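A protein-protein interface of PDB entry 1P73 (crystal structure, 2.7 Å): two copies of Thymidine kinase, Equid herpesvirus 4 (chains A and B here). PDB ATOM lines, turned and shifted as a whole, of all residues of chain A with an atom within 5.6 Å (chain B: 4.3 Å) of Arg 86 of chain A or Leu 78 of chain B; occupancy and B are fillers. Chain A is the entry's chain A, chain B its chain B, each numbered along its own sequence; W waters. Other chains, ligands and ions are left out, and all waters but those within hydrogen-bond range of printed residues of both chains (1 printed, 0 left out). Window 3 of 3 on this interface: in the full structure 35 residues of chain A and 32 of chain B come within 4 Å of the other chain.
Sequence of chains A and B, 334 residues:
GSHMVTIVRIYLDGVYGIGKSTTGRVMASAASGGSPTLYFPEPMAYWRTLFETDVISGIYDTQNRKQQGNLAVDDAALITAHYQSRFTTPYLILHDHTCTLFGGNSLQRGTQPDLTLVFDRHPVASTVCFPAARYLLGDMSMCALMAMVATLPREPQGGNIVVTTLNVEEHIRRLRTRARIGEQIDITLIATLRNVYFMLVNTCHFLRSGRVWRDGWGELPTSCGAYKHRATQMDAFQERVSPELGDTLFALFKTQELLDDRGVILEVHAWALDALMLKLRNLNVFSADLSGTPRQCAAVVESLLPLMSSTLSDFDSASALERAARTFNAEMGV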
ATOM      1  N   TYR A  46      18.862   9.391  32.427  1.00  0.00           N
ATOM      2  CA  TYR A  46      19.446   9.645  31.112  1.00  0.00           C
ATOM      3  C   TYR A  46      19.546  11.140  30.804  1.00  0.00           C
ATOM      4  O   TYR A  46      20.574  11.615  30.329  1.00  0.00           O
ATOM      5  CB  TYR A  46      18.645   8.936  30.014  1.00  0.00           C
ATOM      6  CG  TYR A  46      19.453   8.685  28.771  1.00  0.00           C
ATOM      7  CD1 TYR A  46      19.970   7.415  28.507  1.00  0.00           C
ATOM      8  CD2 TYR A  46      19.724   9.719  27.872  1.00  0.00           C
ATOM      9  CE1 TYR A  46      20.731   7.174  27.380  1.00  0.00           C
ATOM     10  CE2 TYR A  46      20.490   9.497  26.743  1.00  0.00           C
ATOM     11  CZ  TYR A  46      20.990   8.221  26.503  1.00  0.00           C
ATOM     12  OH  TYR A  46      21.745   7.981  25.391  1.00  0.00           O
ATOM     13  N   TRP A  47      18.470  11.865  31.091  1.00  0.00           N
ATOM     14  CA  TRP A  47      18.355  13.289  30.818  1.00  0.00           C
ATOM     15  C   TRP A  47      19.182  14.182  31.750  1.00  0.00           C
ATOM     16  O   TRP A  47      19.699  15.222  31.333  1.00  0.00           O
ATOM     17  CB  TRP A  47      16.898  13.695  30.976  1.00  0.00           C
ATOM     18  CG  TRP A  47      15.969  13.198  29.922  1.00  0.00           C
ATOM     19  CD1 TRP A  47      16.283  12.828  28.650  1.00  0.00           C
ATOM     20  CD2 TRP A  47      14.548  13.036  30.048  1.00  0.00           C
ATOM     21  NE1 TRP A  47      15.150  12.442  27.978  1.00  0.00           N
ATOM     22  CE2 TRP A  47      14.068  12.562  28.812  1.00  0.00           C
ATOM     23  CE3 TRP A  47      13.625  13.251  31.090  1.00  0.00           C
ATOM     24  CZ2 TRP A  47      12.711  12.301  28.581  1.00  0.00           C
ATOM     25  CZ3 TRP A  47      12.279  12.996  30.862  1.00  0.00           C
ATOM     26  CH2 TRP A  47      11.832  12.525  29.614  1.00  0.00           C
ATOM     27  N   THR A  53      25.746  17.282  30.962  1.00  0.00           N
ATOM     28  CA  THR A  53      24.654  18.255  30.850  1.00  0.00           C
ATOM     29  C   THR A  53      23.332  17.738  31.447  1.00  0.00           C
ATOM     30  O   THR A  53      23.081  16.536  31.480  1.00  0.00           O
ATOM     31  CB  THR A  53      24.452  18.676  29.362  1.00  0.00           C
ATOM     32  OG1 THR A  53      25.660  19.247  28.845  1.00  0.00           O
ATOM     33  CG2 THR A  53      23.476  19.834  29.234  1.00  0.00           C
ATOM     34  N   VAL A  55      19.521  18.140  30.548  1.00  0.00           N
ATOM     35  CA  VAL A  55      18.637  18.623  29.484  1.00  0.00           C
ATOM     36  C   VAL A  55      17.390  19.361  29.987  1.00  0.00           C
ATOM     37  O   VAL A  55      16.870  20.224  29.288  1.00  0.00           O
ATOM     38  CB  VAL A  55      18.276  17.517  28.438  1.00  0.00           C
ATOM     39  CG1 VAL A  55      19.486  16.620  28.144  1.00  0.00           C
ATOM     40  CG2 VAL A  55      17.068  16.699  28.873  1.00  0.00           C
ATOM     41  N   LEU A  78      18.130  27.446  18.397  1.00  0.00           N
ATOM     42  CA  LEU A  78      18.949  26.355  17.901  1.00  0.00           C
ATOM     43  C   LEU A  78      19.445  25.488  19.047  1.00  0.00           C
ATOM     44  O   LEU A  78      19.629  24.283  18.880  1.00  0.00           O
ATOM     45  CB  LEU A  78      20.124  26.893  17.081  1.00  0.00           C
ATOM     46  CG  LEU A  78      19.909  27.583  15.716  1.00  0.00           C
ATOM     47  CD1 LEU A  78      20.865  26.982  14.704  1.00  0.00           C
ATOM     48  CD2 LEU A  78      18.472  27.541  15.168  1.00  0.00           C
ATOM     49  N   ILE A  79      19.655  26.094  20.213  1.00  0.00           N
ATOM     50  CA  ILE A  79      20.104  25.340  21.386  1.00  0.00           C
ATOM     51  C   ILE A  79      18.946  24.592  22.046  1.00  0.00           C
ATOM     52  O   ILE A  79      19.115  23.455  22.484  1.00  0.00           O
ATOM     53  CB  ILE A  79      20.865  26.240  22.390  1.00  0.00           C
ATOM     54  CG1 ILE A  79      22.268  26.546  21.853  1.00  0.00           C
ATOM     55  CG2 ILE A  79      20.977  25.569  23.756  1.00  0.00           C
ATOM     56  CD1 ILE A  79      22.952  27.731  22.520  1.00  0.00           C
ATOM     57  N   HIS A  82      18.327  21.542  19.950  1.00  0.00           N
ATOM     58  CA  HIS A  82      19.288  20.467  20.150  1.00  0.00           C
ATOM     59  C   HIS A  82      18.946  19.653  21.387  1.00  0.00           C
ATOM     60  O   HIS A  82      19.076  18.430  21.383  1.00  0.00           O
ATOM     61  CB  HIS A  82      20.701  21.014  20.273  1.00  0.00           C
ATOM     62  CG  HIS A  82      21.683  20.002  20.764  1.00  0.00           C
ATOM     63  ND1 HIS A  82      22.013  18.876  20.039  1.00  0.00           N
ATOM     64  CD2 HIS A  82      22.372  19.919  21.926  1.00  0.00           C
ATOM     65  CE1 HIS A  82      22.879  18.154  20.726  1.00  0.00           C
ATOM     66  NE2 HIS A  82      23.121  18.769  21.871  1.00  0.00           N
ATOM     67  N   TYR A  83      18.525  20.354  22.442  1.00  0.00           N
ATOM     68  CA  TYR A  83      18.119  19.748  23.709  1.00  0.00           C
ATOM     69  C   TYR A  83      16.886  18.868  23.540  1.00  0.00           C
ATOM     70  O   TYR A  83      16.798  17.776  24.095  1.00  0.00           O
ATOM     71  CB  TYR A  83      17.847  20.841  24.750  1.00  0.00           C
ATOM     72  CG  TYR A  83      19.087  21.318  25.461  1.00  0.00           C
ATOM     73  CD1 TYR A  83      19.288  22.669  25.727  1.00  0.00           C
ATOM     74  CD2 TYR A  83      20.069  20.413  25.852  1.00  0.00           C
ATOM     75  CE1 TYR A  83      20.437  23.111  26.382  1.00  0.00           C
ATOM     76  CE2 TYR A  83      21.227  20.839  26.501  1.00  0.00           C
ATOM     77  CZ  TYR A  83      21.405  22.188  26.766  1.00  0.00           C
ATOM     78  OH  TYR A  83      22.553  22.590  27.408  1.00  0.00           O
ATOM     79  N   GLN A  84      15.934  19.362  22.765  1.00  0.00           N
ATOM     80  CA  GLN A  84      14.804  18.560  22.355  1.00  0.00           C
ATOM     81  C   GLN A  84      15.284  17.218  21.775  1.00  0.00           C
ATOM     82  O   GLN A  84      14.757  16.174  22.145  1.00  0.00           O
ATOM     83  CB  GLN A  84      13.935  19.345  21.374  1.00  0.00           C
ATOM     84  CG  GLN A  84      12.422  19.048  21.423  1.00  0.00           C
ATOM     85  CD  GLN A  84      11.841  18.787  22.820  1.00  0.00           C
ATOM     86  OE1 GLN A  84      11.378  19.712  23.491  1.00  0.00           O
ATOM     87  NE2 GLN A  84      11.827  17.521  23.232  1.00  0.00           N
ATOM     88  N   SER A  85      16.300  17.232  20.912  1.00  0.00           N
ATOM     89  CA  SER A  85      16.871  15.983  20.387  1.00  0.00           C
ATOM     90  C   SER A  85      17.290  15.039  21.507  1.00  0.00           C
ATOM     91  O   SER A  85      17.069  13.833  21.426  1.00  0.00           O
ATOM     92  CB  SER A  85      18.079  16.240  19.483  1.00  0.00           C
ATOM     93  OG  SER A  85      17.741  17.089  18.411  1.00  0.00           O
ATOM     94  N   ARG A  86      17.886  15.604  22.553  1.00  0.00           N
ATOM     95  CA  ARG A  86      18.449  14.822  23.656  1.00  0.00           C
ATOM     96  C   ARG A  86      17.388  14.161  24.530  1.00  0.00           C
ATOM     97  O   ARG A  86      17.661  13.143  25.166  1.00  0.00           O
ATOM     98  CB  ARG A  86      19.352  15.697  24.523  1.00  0.00           C
ATOM     99  CG  ARG A  86      20.664  16.067  23.872  1.00  0.00           C
ATOM    100  CD  ARG A  86      21.792  16.310  24.865  1.00  0.00           C
ATOM    101  NE  ARG A  86      22.939  16.938  24.215  1.00  0.00           N
ATOM    102  CZ  ARG A  86      24.057  17.292  24.833  1.00  0.00           C
ATOM    103  NH1 ARG A  86      24.189  17.086  26.138  1.00  0.00           N
ATOM    104  NH2 ARG A  86      25.051  17.855  24.142  1.00  0.00           N
ATOM    105  N   PHE A  87      16.200  14.771  24.570  1.00  0.00           N
ATOM    106  CA  PHE A  87      15.032  14.232  25.253  1.00  0.00           C
ATOM    107  C   PHE A  87      14.622  12.929  24.592  1.00  0.00           C
ATOM    108  O   PHE A  87      14.215  11.979  25.249  1.00  0.00           O
ATOM    109  CB  PHE A  87      13.865  15.218  25.154  1.00  0.00           C
ATOM    110  CG  PHE A  87      13.803  16.204  26.280  1.00  0.00           C
ATOM    111  CD1 PHE A  87      14.259  17.506  26.103  1.00  0.00           C
ATOM    112  CD2 PHE A  87      13.279  15.841  27.511  1.00  0.00           C
ATOM    113  CE1 PHE A  87      14.208  18.430  27.140  1.00  0.00           C
ATOM    114  CE2 PHE A  87      13.228  16.754  28.550  1.00  0.00           C
ATOM    115  CZ  PHE A  87      13.700  18.057  28.361  1.00  0.00           C
ATOM    116  N   THR A  88      14.757  12.920  23.272  1.00  0.00           N
ATOM    117  CA  THR A  88      14.295  11.848  22.402  1.00  0.00           C
ATOM    118  C   THR A  88      15.179  10.607  22.498  1.00  0.00           C
ATOM    119  O   THR A  88      14.681   9.490  22.522  1.00  0.00           O
ATOM    120  CB  THR A  88      14.264  12.391  20.958  1.00  0.00           C
ATOM    121  OG1 THR A  88      13.131  13.250  20.789  1.00  0.00           O
ATOM    122  CG2 THR A  88      14.041  11.291  19.954  1.00  0.00           C
ATOM    123  N   THR A  89      16.491  10.804  22.550  1.00  0.00           N
ATOM    124  CA  THR A  89      17.444   9.684  22.580  1.00  0.00           C
ATOM    125  C   THR A  89      17.012   8.439  23.394  1.00  0.00           C
ATOM    126  O   THR A  89      16.852   7.374  22.819  1.00  0.00           O
ATOM    127  CB  THR A  89      18.859  10.163  22.971  1.00  0.00           C
ATOM    128  OG1 THR A  89      19.206  11.290  22.158  1.00  0.00           O
ATOM    129  CG2 THR A  89      19.907   9.107  22.605  1.00  0.00           C
ATOM    130  N   PRO A  90      16.810   8.542  24.703  1.00  0.00           N
ATOM    131  CA  PRO A  90      16.462   7.347  25.477  1.00  0.00           C
ATOM    132  C   PRO A  90      15.125   6.722  25.041  1.00  0.00           C
ATOM    133  O   PRO A  90      14.919   5.517  25.246  1.00  0.00           O
ATOM    134  CB  PRO A  90      16.397   7.863  26.918  1.00  0.00           C
ATOM    135  CG  PRO A  90      16.145   9.322  26.809  1.00  0.00           C
ATOM    136  CD  PRO A  90      16.879   9.744  25.559  1.00  0.00           C
ATOM    137  N   ASP B  74      31.161  25.557  25.018  1.00  0.00           N
ATOM    138  CA  ASP B  74      29.999  24.797  25.482  1.00  0.00           C
ATOM    139  C   ASP B  74      28.804  25.019  24.559  1.00  0.00           C
ATOM    140  O   ASP B  74      28.017  24.100  24.325  1.00  0.00           O
ATOM    141  CB  ASP B  74      29.636  25.176  26.923  1.00  0.00           C
ATOM    142  CG  ASP B  74      30.644  24.650  27.948  1.00  0.00           C
ATOM    143  OD1 ASP B  74      31.099  23.485  27.820  1.00  0.00           O
ATOM    144  OD2 ASP B  74      31.035  25.335  28.919  1.00  0.00           O
ATOM    145  N   ASP B  75      28.681  26.241  24.045  1.00  0.00           N
ATOM    146  CA  ASP B  75      27.664  26.577  23.054  1.00  0.00           C
ATOM    147  C   ASP B  75      28.043  26.046  21.666  1.00  0.00           C
ATOM    148  O   ASP B  75      27.173  25.618  20.908  1.00  0.00           O
ATOM    149  CB  ASP B  75      27.458  28.095  22.996  1.00  0.00           C
ATOM    150  CG  ASP B  75      26.252  28.563  23.805  1.00  0.00           C
ATOM    151  OD1 ASP B  75      25.588  29.525  23.366  1.00  0.00           O
ATOM    152  OD2 ASP B  75      25.895  28.053  24.891  1.00  0.00           O
ATOM    153  N   ALA B  76      29.339  26.075  21.349  1.00  0.00           N
ATOM    154  CA  ALA B  76      29.860  25.663  20.042  1.00  0.00           C
ATOM    155  C   ALA B  76      29.732  24.164  19.774  1.00  0.00           C
ATOM    156  O   ALA B  76      29.713  23.734  18.620  1.00  0.00           O
ATOM    157  CB  ALA B  76      31.313  26.105  19.880  1.00  0.00           C
ATOM    158  N   ALA B  77      29.661  23.371  20.835  1.00  0.00           N
ATOM    159  CA  ALA B  77      29.380  21.949  20.686  1.00  0.00           C
ATOM    160  C   ALA B  77      27.876  21.699  20.511  1.00  0.00           C
ATOM    161  O   ALA B  77      27.475  20.611  20.081  1.00  0.00           O
ATOM    162  CB  ALA B  77      29.931  21.162  21.878  1.00  0.00           C
ATOM    163  N   LEU B  78      27.060  22.709  20.829  1.00  0.00           N
ATOM    164  CA  LEU B  78      25.603  22.571  20.844  1.00  0.00           C
ATOM    165  C   LEU B  78      24.924  22.985  19.537  1.00  0.00           C
ATOM    166  O   LEU B  78      23.979  22.320  19.087  1.00  0.00           O
ATOM    167  CB  LEU B  78      24.993  23.353  22.012  1.00  0.00           C
ATOM    168  CG  LEU B  78      25.228  22.888  23.451  1.00  0.00           C
ATOM    169  CD1 LEU B  78      24.185  23.495  24.383  1.00  0.00           C
ATOM    170  CD2 LEU B  78      25.279  21.365  23.586  1.00  0.00           C
ATOM    171  N   ILE B  79      25.386  24.086  18.942  1.00  0.00           N
ATOM    172  CA  ILE B  79      24.856  24.541  17.653  1.00  0.00           C
ATOM    173  C   ILE B  79      25.453  23.739  16.487  1.00  0.00           C
ATOM    174  O   ILE B  79      24.788  23.538  15.470  1.00  0.00           O
ATOM    175  CB  ILE B  79      25.037  26.071  17.465  1.00  0.00           C
ATOM    176  CG1 ILE B  79      24.309  26.835  18.569  1.00  0.00           C
ATOM    177  CG2 ILE B  79      24.471  26.534  16.133  1.00  0.00           C
ATOM    178  CD1 ILE B  79      25.211  27.757  19.372  1.00  0.00           C
ATOM    179  N   THR B  80      26.693  23.274  16.643  1.00  0.00           N
ATOM    180  CA  THR B  80      27.287  22.338  15.693  1.00  0.00           C
ATOM    181  C   THR B  80      26.393  21.125  15.578  1.00  0.00           C
ATOM    182  O   THR B  80      26.018  20.715  14.475  1.00  0.00           O
ATOM    183  CB  THR B  80      28.671  21.879  16.179  1.00  0.00           C
ATOM    184  OG1 THR B  80      29.523  23.019  16.330  1.00  0.00           O
ATOM    185  CG2 THR B  80      29.380  21.019  15.112  1.00  0.00           C
ATOM    186  N   ALA B  81      26.060  20.566  16.741  1.00  0.00           N
ATOM    187  CA  ALA B  81      25.275  19.344  16.852  1.00  0.00           C
ATOM    188  C   ALA B  81      23.930  19.480  16.160  1.00  0.00           C
ATOM    189  O   ALA B  81      23.485  18.555  15.475  1.00  0.00           O
ATOM    190  CB  ALA B  81      25.085  18.975  18.309  1.00  0.00           C
ATOM    191  N   HIS B  82      23.296  20.637  16.329  1.00  0.00           N
ATOM    192  CA  HIS B  82      22.004  20.884  15.706  1.00  0.00           C
ATOM    193  C   HIS B  82      22.068  20.872  14.164  1.00  0.00           C
ATOM    194  O   HIS B  82      21.182  20.315  13.505  1.00  0.00           O
ATOM    195  CB  HIS B  82      21.367  22.166  16.237  1.00  0.00           C
ATOM    196  CG  HIS B  82      20.032  22.454  15.637  1.00  0.00           C
ATOM    197  ND1 HIS B  82      18.901  21.743  15.970  1.00  0.00           N
ATOM    198  CD2 HIS B  82      19.652  23.351  14.694  1.00  0.00           C
ATOM    199  CE1 HIS B  82      17.876  22.199  15.270  1.00  0.00           C
ATOM    200  NE2 HIS B  82      18.305  23.175  14.489  1.00  0.00           N
ATOM    201  N   SER B 141      30.268  15.701  21.780  1.00  0.00           N
ATOM    202  CA  SER B 141      30.325  14.787  22.925  1.00  0.00           C
ATOM    203  C   SER B 141      29.746  13.387  22.636  1.00  0.00           C
ATOM    204  O   SER B 141      29.113  13.162  21.612  1.00  0.00           O
ATOM    205  CB  SER B 141      29.678  15.427  24.163  1.00  0.00           C
ATOM    206  OG  SER B 141      28.275  15.280  24.136  1.00  0.00           O
ATOM    207  N   CYS B 143      27.312  12.148  24.295  1.00  0.00           N
ATOM    208  CA  CYS B 143      25.880  12.303  24.466  1.00  0.00           C
ATOM    209  C   CYS B 143      25.265  12.815  23.179  1.00  0.00           C
ATOM    210  O   CYS B 143      24.148  12.429  22.822  1.00  0.00           O
ATOM    211  CB  CYS B 143      25.586  13.260  25.625  1.00  0.00           C
ATOM    212  SG  CYS B 143      23.829  13.564  25.929  1.00  0.00           S
HETATM  213  O   HOH W   1      22.873  15.691  28.086  1.00  0.00           O
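SG of Cys 143 of chain B is in hydrogen-bond range of NH1 of Arg 86 of chain A, at 3.5 Å.
OG of Ser 141 of chain B lies close to N of Cys 143 of chain B (3.3 Å). The guanidinium group of Arg 86 of chain A lies within hydrogen-bond range of a ring nitrogen (NE2) of His 82 of chain A (3.0 Å).
Among the printed residues, merely in contact across the chains: Leu 78 of chain A with Ile 79 of chain B (3.9 Å), Leu 78 of chain A with His 82 of chain B (3.7 Å), Ile 79 of chain A with Asp 75 of chain B (3.3 Å), Ile 79 of chain A with Leu 78 of chain B (3.9 Å), Ile 79 of chain A with Ile 79 of chain B (3.9 Å), His 82 of chain A with Leu 78 of chain B (3.6 Å), His 82 of chain A with Ala 81 of chain B (3.4 Å), Tyr 83 of chain A with Leu 78 of chain B (3.6 Å) and Arg 86 of chain A with Leu 78 of chain B (3.6 Å).
Of the printed residues of chain B, Tyr 83 of chain A touches Leu 78 (3.6 Å). Of chain B, only Leu 78 and Cys 143 come within 4 Å of Arg 86 of chain A. Printed residues of chain A within 4 Å of Asp 75 of chain B: Ile 79. Of chain A, only Ile 79, His 82, Tyr 83 and Arg 86 come within 4 Å of Leu 78 of chain B. Printed residues of chain A within 4 Å of Ile 79 of chain B: Leu 78 (3.9 Å) and Ile 79 (3.9 Å). Of the printed residues of chain A, Ala 81 of chain B touches His 82. Printed residues of chain A within 4 Å of His 82 of chain B: Leu 78.
Along chain B the printed residues that touch a printed residue of chain A span positions 75 to 143. Hydrophobic or aromatic side chains of chain A that line the printed part of chain B: Leu 78, Ile 79, His 82 and Tyr 83. Among the printed residues, 10 pairs touch across the chains.
Leu 78 of chain A touches Ile 79 of chain B, and with the chains exchanged Ile 79 of chain A touches Leu 78 of chain B. Leu 78 of chain A touches His 82 of chain B, and with the chains exchanged His 82 of chain A touches Leu 78 of chain B. Ile 79 of chain B touches its own counterpart, Ile 79 of chain A. 3 positions are printed for both chains.
Water W1 lies within hydrogen-bond range of the guanidinium group of Arg 86 of chain A (2.7 Å) and the side-chain sulfur of Cys 143 of chain B (3.2 Å).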
